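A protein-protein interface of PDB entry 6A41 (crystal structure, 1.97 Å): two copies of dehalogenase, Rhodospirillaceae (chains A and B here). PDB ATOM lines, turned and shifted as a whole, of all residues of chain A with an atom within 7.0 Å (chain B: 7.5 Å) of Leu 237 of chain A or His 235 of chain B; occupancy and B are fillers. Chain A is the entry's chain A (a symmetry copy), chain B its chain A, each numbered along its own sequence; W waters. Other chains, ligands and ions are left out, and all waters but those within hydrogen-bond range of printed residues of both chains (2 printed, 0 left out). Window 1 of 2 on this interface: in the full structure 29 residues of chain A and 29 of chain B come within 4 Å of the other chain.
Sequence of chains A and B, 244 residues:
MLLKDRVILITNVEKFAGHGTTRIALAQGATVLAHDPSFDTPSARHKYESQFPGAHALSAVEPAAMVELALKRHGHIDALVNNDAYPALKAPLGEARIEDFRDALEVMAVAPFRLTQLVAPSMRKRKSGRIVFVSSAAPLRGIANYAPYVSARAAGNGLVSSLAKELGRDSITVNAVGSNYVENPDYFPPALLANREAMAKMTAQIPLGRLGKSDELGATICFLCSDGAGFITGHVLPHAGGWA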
ATOM      1  N   ALA A 137     -33.657  -2.610  11.873  1.00  0.00           N
ATOM      2  CA  ALA A 137     -32.352  -2.736  12.516  1.00  0.00           C
ATOM      3  C   ALA A 137     -32.101  -1.640  13.612  1.00  0.00           C
ATOM      4  O   ALA A 137     -31.073  -1.684  14.286  1.00  0.00           O
ATOM      5  CB  ALA A 137     -31.154  -2.759  11.514  1.00  0.00           C
ATOM      6  N   LEU A 140     -30.763  -2.263  17.084  1.00  0.00           N
ATOM      7  CA  LEU A 140     -29.407  -2.849  17.219  1.00  0.00           C
ATOM      8  C   LEU A 140     -28.334  -1.770  17.443  1.00  0.00           C
ATOM      9  O   LEU A 140     -27.183  -2.107  17.774  1.00  0.00           O
ATOM     10  CB  LEU A 140     -29.064  -3.701  15.987  1.00  0.00           C
ATOM     11  CG  LEU A 140     -30.020  -4.912  15.882  1.00  0.00           C
ATOM     12  CD1 LEU A 140     -29.809  -5.601  14.481  1.00  0.00           C
ATOM     13  CD2 LEU A 140     -29.976  -5.806  17.092  1.00  0.00           C
ATOM     14  N   ASN A 175     -39.039 -15.699  12.626  1.00  0.00           N
ATOM     15  CA  ASN A 175     -37.862 -14.805  12.454  1.00  0.00           C
ATOM     16  C   ASN A 175     -38.324 -13.363  12.170  1.00  0.00           C
ATOM     17  O   ASN A 175     -39.511 -13.102  11.852  1.00  0.00           O
ATOM     18  CB  ASN A 175     -37.047 -15.292  11.253  1.00  0.00           C
ATOM     19  CG  ASN A 175     -36.423 -16.643  11.495  1.00  0.00           C
ATOM     20  OD1 ASN A 175     -36.812 -17.652  10.811  1.00  0.00           O
ATOM     21  ND2 ASN A 175     -35.612 -16.773  12.442  1.00  0.00           N
ATOM     22  N   ALA A 176     -37.364 -12.422  12.207  1.00  0.00           N
ATOM     23  CA  ALA A 176     -37.626 -11.055  11.771  1.00  0.00           C
ATOM     24  C   ALA A 176     -36.530 -10.625  10.847  1.00  0.00           C
ATOM     25  O   ALA A 176     -35.367 -11.144  10.921  1.00  0.00           O
ATOM     26  CB  ALA A 176     -37.651 -10.105  12.940  1.00  0.00           C
ATOM     27  N   VAL A 177     -36.821  -9.687   9.983  1.00  0.00           N
ATOM     28  CA  VAL A 177     -35.769  -9.045   9.175  1.00  0.00           C
ATOM     29  C   VAL A 177     -35.712  -7.597   9.721  1.00  0.00           C
ATOM     30  O   VAL A 177     -36.677  -6.916   9.756  1.00  0.00           O
ATOM     31  CB  VAL A 177     -36.124  -9.004   7.690  1.00  0.00           C
ATOM     32  CG1 VAL A 177     -34.999  -8.222   6.921  1.00  0.00           C
ATOM     33  CG2 VAL A 177     -36.146 -10.430   7.111  1.00  0.00           C
ATOM     34  N   GLY A 178     -34.544  -7.187  10.187  1.00  0.00           N
ATOM     35  CA  GLY A 178     -34.296  -5.899  10.755  1.00  0.00           C
ATOM     36  C   GLY A 178     -33.805  -4.983   9.667  1.00  0.00           C
ATOM     37  O   GLY A 178     -32.606  -4.867   9.432  1.00  0.00           O
ATOM     38  N   SER A 179     -34.720  -4.438   8.936  1.00  0.00           N
ATOM     39  CA  SER A 179     -34.328  -3.522   7.833  1.00  0.00           C
ATOM     40  C   SER A 179     -33.867  -2.164   8.282  1.00  0.00           C
ATOM     41  O   SER A 179     -34.279  -1.631   9.304  1.00  0.00           O
ATOM     42  CB  SER A 179     -35.507  -3.289   6.868  1.00  0.00           C
ATOM     43  OG  SER A 179     -35.102  -2.758   5.611  1.00  0.00           O
ATOM     44  N   LEU A 217     -34.575  -6.559   0.052  1.00  0.00           N
ATOM     45  CA  LEU A 217     -35.431  -6.874   1.271  1.00  0.00           C
ATOM     46  C   LEU A 217     -36.420  -7.966   0.936  1.00  0.00           C
ATOM     47  O   LEU A 217     -36.584  -8.911   1.735  1.00  0.00           O
ATOM     48  CB  LEU A 217     -36.093  -5.623   1.750  1.00  0.00           C
ATOM     49  CG  LEU A 217     -36.927  -5.712   3.027  1.00  0.00           C
ATOM     50  CD1 LEU A 217     -36.213  -6.343   4.135  1.00  0.00           C
ATOM     51  CD2 LEU A 217     -37.346  -4.341   3.475  1.00  0.00           C
ATOM     52  N   THR A 220     -34.728 -11.354   0.794  1.00  0.00           N
ATOM     53  CA  THR A 220     -34.452 -11.806   2.173  1.00  0.00           C
ATOM     54  C   THR A 220     -35.615 -12.423   2.875  1.00  0.00           C
ATOM     55  O   THR A 220     -35.537 -13.487   3.489  1.00  0.00           O
ATOM     56  CB  THR A 220     -33.743 -10.681   2.955  1.00  0.00           C
ATOM     57  OG1 THR A 220     -32.535 -10.277   2.218  1.00  0.00           O
ATOM     58  CG2 THR A 220     -33.364 -11.188   4.264  1.00  0.00           C
ATOM     59  N   ILE A 221     -36.718 -11.720   2.846  1.00  0.00           N
ATOM     60  CA  ILE A 221     -37.973 -12.243   3.386  1.00  0.00           C
ATOM     61  C   ILE A 221     -38.393 -13.535   2.698  1.00  0.00           C
ATOM     62  O   ILE A 221     -38.746 -14.549   3.421  1.00  0.00           O
ATOM     63  CB  ILE A 221     -39.054 -11.134   3.343  1.00  0.00           C
ATOM     64  CG1 ILE A 221     -38.727  -9.915   4.174  1.00  0.00           C
ATOM     65  CG2 ILE A 221     -40.445 -11.695   3.588  1.00  0.00           C
ATOM     66  CD1 ILE A 221     -39.486  -8.638   3.711  1.00  0.00           C
ATOM     67  N   PHE A 223     -36.399 -15.685   1.179  1.00  0.00           N
ATOM     68  CA  PHE A 223     -35.531 -16.719   1.643  1.00  0.00           C
ATOM     69  C   PHE A 223     -36.027 -17.304   3.030  1.00  0.00           C
ATOM     70  O   PHE A 223     -36.148 -18.570   3.147  1.00  0.00           O
ATOM     71  CB  PHE A 223     -34.051 -16.237   1.767  1.00  0.00           C
ATOM     72  CG  PHE A 223     -33.178 -17.272   2.540  1.00  0.00           C
ATOM     73  CD1 PHE A 223     -32.905 -18.493   1.978  1.00  0.00           C
ATOM     74  CD2 PHE A 223     -32.758 -16.986   3.833  1.00  0.00           C
ATOM     75  CE1 PHE A 223     -32.192 -19.523   2.689  1.00  0.00           C
ATOM     76  CE2 PHE A 223     -32.030 -17.923   4.560  1.00  0.00           C
ATOM     77  CZ  PHE A 223     -31.765 -19.152   3.997  1.00  0.00           C
ATOM     78  N   LEU A 224     -36.390 -16.461   3.997  1.00  0.00           N
ATOM     79  CA  LEU A 224     -36.820 -16.987   5.297  1.00  0.00           C
ATOM     80  C   LEU A 224     -38.139 -17.757   5.198  1.00  0.00           C
ATOM     81  O   LEU A 224     -38.334 -18.683   6.005  1.00  0.00           O
ATOM     82  CB  LEU A 224     -36.955 -15.888   6.344  1.00  0.00           C
ATOM     83  CG  LEU A 224     -35.577 -15.263   6.643  1.00  0.00           C
ATOM     84  CD1 LEU A 224     -35.822 -13.968   7.407  1.00  0.00           C
ATOM     85  CD2 LEU A 224     -34.638 -16.217   7.401  1.00  0.00           C
ATOM     86  N   ILE A 232     -33.475 -22.082  10.455  1.00  0.00           N
ATOM     87  CA  ILE A 232     -33.254 -20.794  11.005  1.00  0.00           C
ATOM     88  C   ILE A 232     -34.525 -20.400  11.772  1.00  0.00           C
ATOM     89  O   ILE A 232     -35.617 -20.377  11.187  1.00  0.00           O
ATOM     90  CB  ILE A 232     -33.010 -19.738   9.914  1.00  0.00           C
ATOM     91  CG1 ILE A 232     -31.776 -20.172   9.133  1.00  0.00           C
ATOM     92  CG2 ILE A 232     -32.944 -18.336  10.498  1.00  0.00           C
ATOM     93  CD1 ILE A 232     -31.527 -19.349   7.858  1.00  0.00           C
ATOM     94  N   HIS A 235     -34.586 -15.636  15.006  1.00  0.00           N
ATOM     95  CA  HIS A 235     -33.521 -14.757  14.662  1.00  0.00           C
ATOM     96  C   HIS A 235     -34.047 -13.411  14.128  1.00  0.00           C
ATOM     97  O   HIS A 235     -35.008 -13.384  13.380  1.00  0.00           O
ATOM     98  CB  HIS A 235     -32.622 -15.362  13.566  1.00  0.00           C
ATOM     99  CG  HIS A 235     -31.376 -14.536  13.267  1.00  0.00           C
ATOM    100  ND1 HIS A 235     -30.486 -14.112  14.242  1.00  0.00           N
ATOM    101  CD2 HIS A 235     -30.887 -14.086  12.083  1.00  0.00           C
ATOM    102  CE1 HIS A 235     -29.481 -13.452  13.642  1.00  0.00           C
ATOM    103  NE2 HIS A 235     -29.698 -13.434  12.328  1.00  0.00           N
ATOM    104  N   VAL A 236     -33.303 -12.348  14.438  1.00  0.00           N
ATOM    105  CA  VAL A 236     -33.539 -11.021  13.811  1.00  0.00           C
ATOM    106  C   VAL A 236     -32.364 -10.718  12.845  1.00  0.00           C
ATOM    107  O   VAL A 236     -31.250 -10.496  13.327  1.00  0.00           O
ATOM    108  CB  VAL A 236     -33.609  -9.924  14.902  1.00  0.00           C
ATOM    109  CG1 VAL A 236     -33.739  -8.581  14.158  1.00  0.00           C
ATOM    110  CG2 VAL A 236     -34.758 -10.237  15.813  1.00  0.00           C
ATOM    111  N   LEU A 237     -32.593 -10.865  11.548  1.00  0.00           N
ATOM    112  CA  LEU A 237     -31.601 -10.782  10.487  1.00  0.00           C
ATOM    113  C   LEU A 237     -31.465  -9.314  10.044  1.00  0.00           C
ATOM    114  O   LEU A 237     -32.345  -8.741   9.361  1.00  0.00           O
ATOM    115  CB  LEU A 237     -31.995 -11.679   9.355  1.00  0.00           C
ATOM    116  CG  LEU A 237     -31.301 -11.691   8.031  1.00  0.00           C
ATOM    117  CD1 LEU A 237     -29.869 -11.593   8.261  1.00  0.00           C
ATOM    118  CD2 LEU A 237     -31.673 -12.985   7.271  1.00  0.00           C
ATOM    119  N   PRO A 238     -30.345  -8.667  10.406  1.00  0.00           N
ATOM    120  CA  PRO A 238     -30.093  -7.293   9.945  1.00  0.00           C
ATOM    121  C   PRO A 238     -29.909  -7.154   8.455  1.00  0.00           C
ATOM    122  O   PRO A 238     -29.217  -7.970   7.790  1.00  0.00           O
ATOM    123  CB  PRO A 238     -28.845  -6.872  10.707  1.00  0.00           C
ATOM    124  CG  PRO A 238     -28.700  -7.988  11.685  1.00  0.00           C
ATOM    125  CD  PRO A 238     -29.184  -9.205  11.068  1.00  0.00           C
ATOM    126  N   HIS A 239     -30.624  -6.193   7.899  1.00  0.00           N
ATOM    127  CA  HIS A 239     -30.664  -5.961   6.471  1.00  0.00           C
ATOM    128  C   HIS A 239     -30.575  -4.458   6.258  1.00  0.00           C
ATOM    129  O   HIS A 239     -31.480  -3.819   5.933  1.00  0.00           O
ATOM    130  CB  HIS A 239     -31.947  -6.542   5.897  1.00  0.00           C
ATOM    131  CG  HIS A 239     -31.996  -6.509   4.419  1.00  0.00           C
ATOM    132  ND1 HIS A 239     -32.362  -5.378   3.735  1.00  0.00           N
ATOM    133  CD2 HIS A 239     -31.689  -7.447   3.492  1.00  0.00           C
ATOM    134  CE1 HIS A 239     -32.330  -5.640   2.424  1.00  0.00           C
ATOM    135  NE2 HIS A 239     -31.952  -6.888   2.241  1.00  0.00           N
ATOM    136  N   ALA A 240     -29.332  -3.967   6.446  1.00  0.00           N
ATOM    137  CA  ALA A 240     -29.066  -2.562   6.477  1.00  0.00           C
ATOM    138  C   ALA A 240     -27.713  -2.191   5.946  1.00  0.00           C
ATOM    139  O   ALA A 240     -27.155  -1.201   6.390  1.00  0.00           O
ATOM    140  CB  ALA A 240     -29.177  -2.109   7.908  1.00  0.00           C
ATOM    141  N   GLY A 242     -24.778  -3.280   6.292  1.00  0.00           N
ATOM    142  CA  GLY A 242     -23.699  -3.259   7.306  1.00  0.00           C
ATOM    143  C   GLY A 242     -23.837  -2.224   8.466  1.00  0.00           C
ATOM    144  O   GLY A 242     -23.039  -2.231   9.373  1.00  0.00           O
ATOM    145  N   ALA A 244     -25.852  -2.237  10.859  1.00  0.00           N
ATOM    146  CA  ALA A 244     -25.930  -3.075  12.100  1.00  0.00           C
ATOM    147  C   ALA A 244     -25.662  -4.599  11.769  1.00  0.00           C
ATOM    148  O   ALA A 244     -25.892  -4.757  10.401  1.00  0.00           O
ATOM    149  CB  ALA A 244     -27.305  -2.971  12.622  1.00  0.00           C
ATOM    150  N   ILE B 131     -18.110 -13.062   0.294  1.00  0.00           N
ATOM    151  CA  ILE B 131     -17.271 -13.951   1.076  1.00  0.00           C
ATOM    152  C   ILE B 131     -18.131 -14.528   2.243  1.00  0.00           C
ATOM    153  O   ILE B 131     -18.755 -13.708   2.983  1.00  0.00           O
ATOM    154  CB  ILE B 131     -16.099 -13.176   1.726  1.00  0.00           C
ATOM    155  CG1 ILE B 131     -15.200 -12.348   0.822  1.00  0.00           C
ATOM    156  CG2 ILE B 131     -15.238 -14.106   2.575  1.00  0.00           C
ATOM    157  CD1 ILE B 131     -14.282 -13.107   0.045  1.00  0.00           C
ATOM    158  N   PHE B 133     -18.025 -17.076   5.530  1.00  0.00           N
ATOM    159  CA  PHE B 133     -17.352 -17.953   6.435  1.00  0.00           C
ATOM    160  C   PHE B 133     -18.317 -18.997   6.910  1.00  0.00           C
ATOM    161  O   PHE B 133     -19.389 -18.672   7.541  1.00  0.00           O
ATOM    162  CB  PHE B 133     -16.709 -17.165   7.588  1.00  0.00           C
ATOM    163  CG  PHE B 133     -15.576 -16.254   7.172  1.00  0.00           C
ATOM    164  CD1 PHE B 133     -15.828 -15.011   6.637  1.00  0.00           C
ATOM    165  CD2 PHE B 133     -14.282 -16.591   7.403  1.00  0.00           C
ATOM    166  CE1 PHE B 133     -14.805 -14.143   6.272  1.00  0.00           C
ATOM    167  CE2 PHE B 133     -13.238 -15.725   7.000  1.00  0.00           C
ATOM    168  CZ  PHE B 133     -13.533 -14.542   6.389  1.00  0.00           C
ATOM    169  N   ASN B 157     -15.570 -15.687  13.564  1.00  0.00           N
ATOM    170  CA  ASN B 157     -16.699 -14.798  13.486  1.00  0.00           C
ATOM    171  C   ASN B 157     -16.246 -13.329  13.601  1.00  0.00           C
ATOM    172  O   ASN B 157     -16.859 -12.439  13.059  1.00  0.00           O
ATOM    173  CB  ASN B 157     -17.752 -15.090  14.590  1.00  0.00           C
ATOM    174  CG  ASN B 157     -18.480 -16.400  14.358  1.00  0.00           C
ATOM    175  OD1 ASN B 157     -18.384 -17.007  13.287  1.00  0.00           O
ATOM    176  ND2 ASN B 157     -19.171 -16.881  15.369  1.00  0.00           N
ATOM    177  N   VAL B 160     -15.537 -10.833  10.560  1.00  0.00           N
ATOM    178  CA  VAL B 160     -16.585 -10.590   9.619  1.00  0.00           C
ATOM    179  C   VAL B 160     -16.949  -9.140   9.538  1.00  0.00           C
ATOM    180  O   VAL B 160     -16.868  -8.596   8.433  1.00  0.00           O
ATOM    181  CB  VAL B 160     -17.773 -11.497   9.951  1.00  0.00           C
ATOM    182  CG1 VAL B 160     -19.020 -11.144   9.185  1.00  0.00           C
ATOM    183  CG2 VAL B 160     -17.434 -12.977   9.627  1.00  0.00           C
ATOM    184  N   SER B 161     -17.273  -8.487  10.667  1.00  0.00           N
ATOM    185  CA  SER B 161     -17.710  -7.127  10.534  1.00  0.00           C
ATOM    186  C   SER B 161     -16.579  -6.162  10.086  1.00  0.00           C
ATOM    187  O   SER B 161     -16.812  -5.160   9.368  1.00  0.00           O
ATOM    188  CB  SER B 161     -18.370  -6.662  11.812  1.00  0.00           C
ATOM    189  OG  SER B 161     -17.497  -6.698  12.902  1.00  0.00           O
ATOM    190  N   ALA B 164     -16.093  -6.741   6.432  1.00  0.00           N
ATOM    191  CA  ALA B 164     -17.228  -6.177   5.739  1.00  0.00           C
ATOM    192  C   ALA B 164     -17.025  -4.665   5.528  1.00  0.00           C
ATOM    193  O   ALA B 164     -17.307  -4.123   4.459  1.00  0.00           O
ATOM    194  CB  ALA B 164     -18.568  -6.440   6.496  1.00  0.00           C
ATOM    195  N   VAL B 174     -19.457  -9.570   3.185  1.00  0.00           N
ATOM    196  CA  VAL B 174     -18.745 -10.512   4.004  1.00  0.00           C
ATOM    197  C   VAL B 174     -19.686 -10.881   5.158  1.00  0.00           C
ATOM    198  O   VAL B 174     -20.030 -10.064   5.965  1.00  0.00           O
ATOM    199  CB  VAL B 174     -17.490  -9.958   4.574  1.00  0.00           C
ATOM    200  CG1 VAL B 174     -16.727 -11.038   5.301  1.00  0.00           C
ATOM    201  CG2 VAL B 174     -16.572  -9.380   3.523  1.00  0.00           C
ATOM    202  N   ASN B 175     -19.954 -12.150   5.246  1.00  0.00           N
ATOM    203  CA  ASN B 175     -20.856 -12.704   6.291  1.00  0.00           C
ATOM    204  C   ASN B 175     -20.328 -14.064   6.786  1.00  0.00           C
ATOM    205  O   ASN B 175     -19.437 -14.691   6.161  1.00  0.00           O
ATOM    206  CB  ASN B 175     -22.242 -12.923   5.678  1.00  0.00           C
ATOM    207  CG  ASN B 175     -22.910 -11.627   5.295  1.00  0.00           C
ATOM    208  OD1 ASN B 175     -23.123 -11.364   4.061  1.00  0.00           O
ATOM    209  ND2 ASN B 175     -23.142 -10.780   6.190  1.00  0.00           N
ATOM    210  N   ALA B 176     -20.934 -14.566   7.877  1.00  0.00           N
ATOM    211  CA  ALA B 176     -20.665 -15.924   8.335  1.00  0.00           C
ATOM    212  C   ALA B 176     -21.968 -16.612   8.599  1.00  0.00           C
ATOM    213  O   ALA B 176     -23.012 -15.944   8.906  1.00  0.00           O
ATOM    214  CB  ALA B 176     -19.870 -15.921   9.615  1.00  0.00           C
ATOM    215  N   VAL B 177     -21.974 -17.917   8.519  1.00  0.00           N
ATOM    216  CA  VAL B 177     -23.140 -18.700   8.963  1.00  0.00           C
ATOM    217  C   VAL B 177     -22.631 -19.446  10.221  1.00  0.00           C
ATOM    218  O   VAL B 177     -21.667 -20.129  10.180  1.00  0.00           O
ATOM    219  CB  VAL B 177     -23.581 -19.725   7.920  1.00  0.00           C
ATOM    220  CG1 VAL B 177     -24.760 -20.576   8.511  1.00  0.00           C
ATOM    221  CG2 VAL B 177     -24.132 -19.009   6.674  1.00  0.00           C
ATOM    222  N   GLY B 178     -23.299 -19.238  11.343  1.00  0.00           N
ATOM    223  CA  GLY B 178     -22.970 -19.812  12.610  1.00  0.00           C
ATOM    224  C   GLY B 178     -23.752 -21.087  12.775  1.00  0.00           C
ATOM    225  O   GLY B 178     -24.856 -21.087  13.309  1.00  0.00           O
ATOM    226  N   PHE B 223     -27.930 -18.770  -0.283  1.00  0.00           N
ATOM    227  CA  PHE B 223     -28.630 -17.528  -0.212  1.00  0.00           C
ATOM    228  C   PHE B 223     -27.629 -16.318   0.007  1.00  0.00           C
ATOM    229  O   PHE B 223     -27.716 -15.310  -0.772  1.00  0.00           O
ATOM    230  CB  PHE B 223     -29.719 -17.526   0.907  1.00  0.00           C
ATOM    231  CG  PHE B 223     -30.267 -16.090   1.165  1.00  0.00           C
ATOM    232  CD1 PHE B 223     -31.019 -15.462   0.206  1.00  0.00           C
ATOM    233  CD2 PHE B 223     -29.915 -15.419   2.330  1.00  0.00           C
ATOM    234  CE1 PHE B 223     -31.464 -14.099   0.349  1.00  0.00           C
ATOM    235  CE2 PHE B 223     -30.346 -14.114   2.548  1.00  0.00           C
ATOM    236  CZ  PHE B 223     -31.093 -13.482   1.578  1.00  0.00           C
ATOM    237  N   LEU B 224     -26.672 -16.426   0.929  1.00  0.00           N
ATOM    238  CA  LEU B 224     -25.759 -15.302   1.165  1.00  0.00           C
ATOM    239  C   LEU B 224     -24.850 -15.039  -0.038  1.00  0.00           C
ATOM    240  O   LEU B 224     -24.461 -13.873  -0.228  1.00  0.00           O
ATOM    241  CB  LEU B 224     -24.904 -15.509   2.409  1.00  0.00           C
ATOM    242  CG  LEU B 224     -25.792 -15.527   3.670  1.00  0.00           C
ATOM    243  CD1 LEU B 224     -24.949 -16.081   4.811  1.00  0.00           C
ATOM    244  CD2 LEU B 224     -26.388 -14.149   4.003  1.00  0.00           C
ATOM    245  N   ILE B 232     -26.979  -7.576   2.768  1.00  0.00           N
ATOM    246  CA  ILE B 232     -26.637  -8.167   4.011  1.00  0.00           C
ATOM    247  C   ILE B 232     -25.104  -8.236   4.077  1.00  0.00           C
ATOM    248  O   ILE B 232     -24.474  -8.831   3.191  1.00  0.00           O
ATOM    249  CB  ILE B 232     -27.184  -9.598   4.137  1.00  0.00           C
ATOM    250  CG1 ILE B 232     -28.701  -9.514   4.019  1.00  0.00           C
ATOM    251  CG2 ILE B 232     -26.671 -10.284   5.392  1.00  0.00           C
ATOM    252  CD1 ILE B 232     -29.391 -10.882   3.891  1.00  0.00           C
ATOM    253  N   THR B 233     -24.528  -7.635   5.108  1.00  0.00           N
ATOM    254  CA  THR B 233     -23.013  -7.772   5.277  1.00  0.00           C
ATOM    255  C   THR B 233     -22.650  -7.527   6.687  1.00  0.00           C
ATOM    256  O   THR B 233     -23.409  -6.871   7.441  1.00  0.00           O
ATOM    257  CB  THR B 233     -22.257  -6.803   4.316  1.00  0.00           C
ATOM    258  OG1 THR B 233     -20.921  -7.182   4.189  1.00  0.00           O
ATOM    259  CG2 THR B 233     -22.313  -5.360   4.719  1.00  0.00           C
ATOM    260  N   GLY B 234     -21.530  -8.102   7.080  1.00  0.00           N
ATOM    261  CA  GLY B 234     -21.081  -7.961   8.403  1.00  0.00           C
ATOM    262  C   GLY B 234     -21.802  -8.818   9.412  1.00  0.00           C
ATOM    263  O   GLY B 234     -21.679  -8.555  10.615  1.00  0.00           O
ATOM    264  N   HIS B 235     -22.494  -9.844   8.951  1.00  0.00           N
ATOM    265  CA  HIS B 235     -23.392 -10.516   9.828  1.00  0.00           C
ATOM    266  C   HIS B 235     -22.954 -11.971  10.081  1.00  0.00           C
ATOM    267  O   HIS B 235     -22.516 -12.646   9.166  1.00  0.00           O
ATOM    268  CB  HIS B 235     -24.818 -10.564   9.246  1.00  0.00           C
ATOM    269  CG  HIS B 235     -25.856 -11.133  10.207  1.00  0.00           C
ATOM    270  ND1 HIS B 235     -26.032 -10.672  11.503  1.00  0.00           N
ATOM    271  CD2 HIS B 235     -26.775 -12.115  10.023  1.00  0.00           C
ATOM    272  CE1 HIS B 235     -27.051 -11.349  12.060  1.00  0.00           C
ATOM    273  NE2 HIS B 235     -27.525 -12.224  11.174  1.00  0.00           N
ATOM    274  N   VAL B 236     -23.217 -12.439  11.303  1.00  0.00           N
ATOM    275  CA  VAL B 236     -23.074 -13.880  11.634  1.00  0.00           C
ATOM    276  C   VAL B 236     -24.489 -14.481  11.834  1.00  0.00           C
ATOM    277  O   VAL B 236     -25.142 -14.132  12.822  1.00  0.00           O
ATOM    278  CB  VAL B 236     -22.251 -14.046  12.936  1.00  0.00           C
ATOM    279  CG1 VAL B 236     -22.253 -15.553  13.261  1.00  0.00           C
ATOM    280  CG2 VAL B 236     -20.887 -13.467  12.709  1.00  0.00           C
ATOM    281  N   LEU B 237     -24.977 -15.222  10.851  1.00  0.00           N
ATOM    282  CA  LEU B 237     -26.330 -15.752  10.764  1.00  0.00           C
ATOM    283  C   LEU B 237     -26.380 -17.113  11.481  1.00  0.00           C
ATOM    284  O   LEU B 237     -25.870 -18.145  10.985  1.00  0.00           O
ATOM    285  CB  LEU B 237     -26.743 -15.854   9.329  1.00  0.00           C
ATOM    286  CG  LEU B 237     -27.995 -16.533   8.876  1.00  0.00           C
ATOM    287  CD1 LEU B 237     -29.066 -16.184   9.795  1.00  0.00           C
ATOM    288  CD2 LEU B 237     -28.317 -16.098   7.428  1.00  0.00           C
ATOM    289  N   PRO B 238     -27.014 -17.159  12.664  1.00  0.00           N
ATOM    290  CA  PRO B 238     -27.189 -18.437  13.370  1.00  0.00           C
ATOM    291  C   PRO B 238     -28.067 -19.435  12.655  1.00  0.00           C
ATOM    292  O   PRO B 238     -29.143 -19.095  12.096  1.00  0.00           O
ATOM    293  CB  PRO B 238     -27.774 -18.038  14.715  1.00  0.00           C
ATOM    294  CG  PRO B 238     -27.623 -16.555  14.680  1.00  0.00           C
ATOM    295  CD  PRO B 238     -27.764 -16.112  13.310  1.00  0.00           C
HETATM  296  O   HOH W   1     -24.901  -7.119   9.723  1.00  0.00           O
HETATM  297  O   HOH W   2     -26.510  -7.472   7.513  1.00  0.00           O
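NE2 of His 235 of chain A lies within hydrogen-bond range of NE2 of His 235 of chain B.
The side-chain amide nitrogen of Asn 175 of chain A lies close to the backbone NH of His 235 of chain A, 3.0 Å away. ND2 of Asn 175 of chain B lies close to N of His 235 of chain B (3.0 Å). O of His 235 of chain B sits at hydrogen-bond distance from N of Ala 176 of chain B (2.8 Å). N of Val 174 of chain B is in hydrogen-bond range of OG1 of Thr 233 of chain B, 3.0 Å away. N of Gly 178 of chain A lies within hydrogen-bond range of O of Leu 237 of chain A, at 2.8 Å. The backbone carbonyl oxygen of Gly 178 of chain A sits at hydrogen-bond distance from the backbone NH of His 239 of chain A.
Among the printed residues, merely in contact across the chains: Thr 220 of chain A with Phe 223 of chain B, Thr 220 of chain A with Ile 232 of chain B, Phe 223 of chain A with Phe 223 of chain B, His 235 of chain A with Leu 237 of chain B, His 235 of chain A with Pro 238 of chain B, Leu 237 of chain A with His 235 of chain B, Pro 238 of chain A with His 235 of chain B, His 239 of chain A with Ile 232 of chain B and Gly 242 of chain A with Thr 233 of chain B.
Of the printed residues of chain B, Leu 237 of chain A touches His 235 (3.6 Å). His 235 of chain B touches just these residues of chain A: His 235, Leu 237 and Pro 238. No residue of chain A comes within 4 Å of Gly 234 of chain B. Printed residues of chain B within 4 Å of Pro 238 of chain A: His 235. Of the printed residues of chain A, Thr 233 of chain B touches Gly 242. Printed residues of chain B within 4 Å of Phe 223 of chain A: Phe 223 (3.4 Å). Printed residues of chain A within 4 Å of Phe 223 of chain B: Thr 220 and Phe 223. Of the printed residues of chain B, Gly 242 of chain A touches Thr 233. Ala 244 of chain A touches none of the printed residues of chain B. The nearest printed residue of chain A that does not touch Phe 223 of chain B is Leu 237 of chain A (5.0 Å).
Printed residues of chain A that touch a printed residue of chain B: Thr 220, Phe 223, His 235, Leu 237, Pro 238, His 239 and Gly 242. Hydrophobic or aromatic side chains of chain A within 4 Å of the printed part of chain B: Phe 223, His 235, Leu 237, Pro 238 and His 239. Of the 20 printed residues of chain B, 6 touch a printed residue of chain A. Printed residues of chain B that touch a printed residue of chain A: Phe 223, Ile 232, Thr 233, His 235, Leu 237 and Pro 238. Hydrophobic or aromatic side chains of chain B within 4 Å of the printed part of chain A: Phe 223, Ile 232, His 235, Leu 237 and Pro 238. Among the printed residues, 10 pairs touch across the chains. Among the printed residues, no Asp or Glu carboxylate lies within 4 Å of a Lys or Arg side-chain nitrogen of the other chain.
Phe 223 of chain B touches its own counterpart, Phe 223 of chain A. His 235 of chain B touches its own counterpart, His 235 of chain A. His 235 of chain A touches Leu 237 of chain B, and with the chains exchanged Leu 237 of chain A touches His 235 of chain B. His 235 of chain A touches Pro 238 of chain B, and with the chains exchanged Pro 238 of chain A touches His 235 of chain B. 11 positions are printed for both chains.
Water W1 lies within hydrogen-bond range of O of Ala 244 of chain A (2.6 Å) and O of Thr 233 of chain B (2.7 Å). Water W2 bridges the backbone carbonyl oxygen of Pro 238 of chain A and the backbone NH of Thr 233 of chain B.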
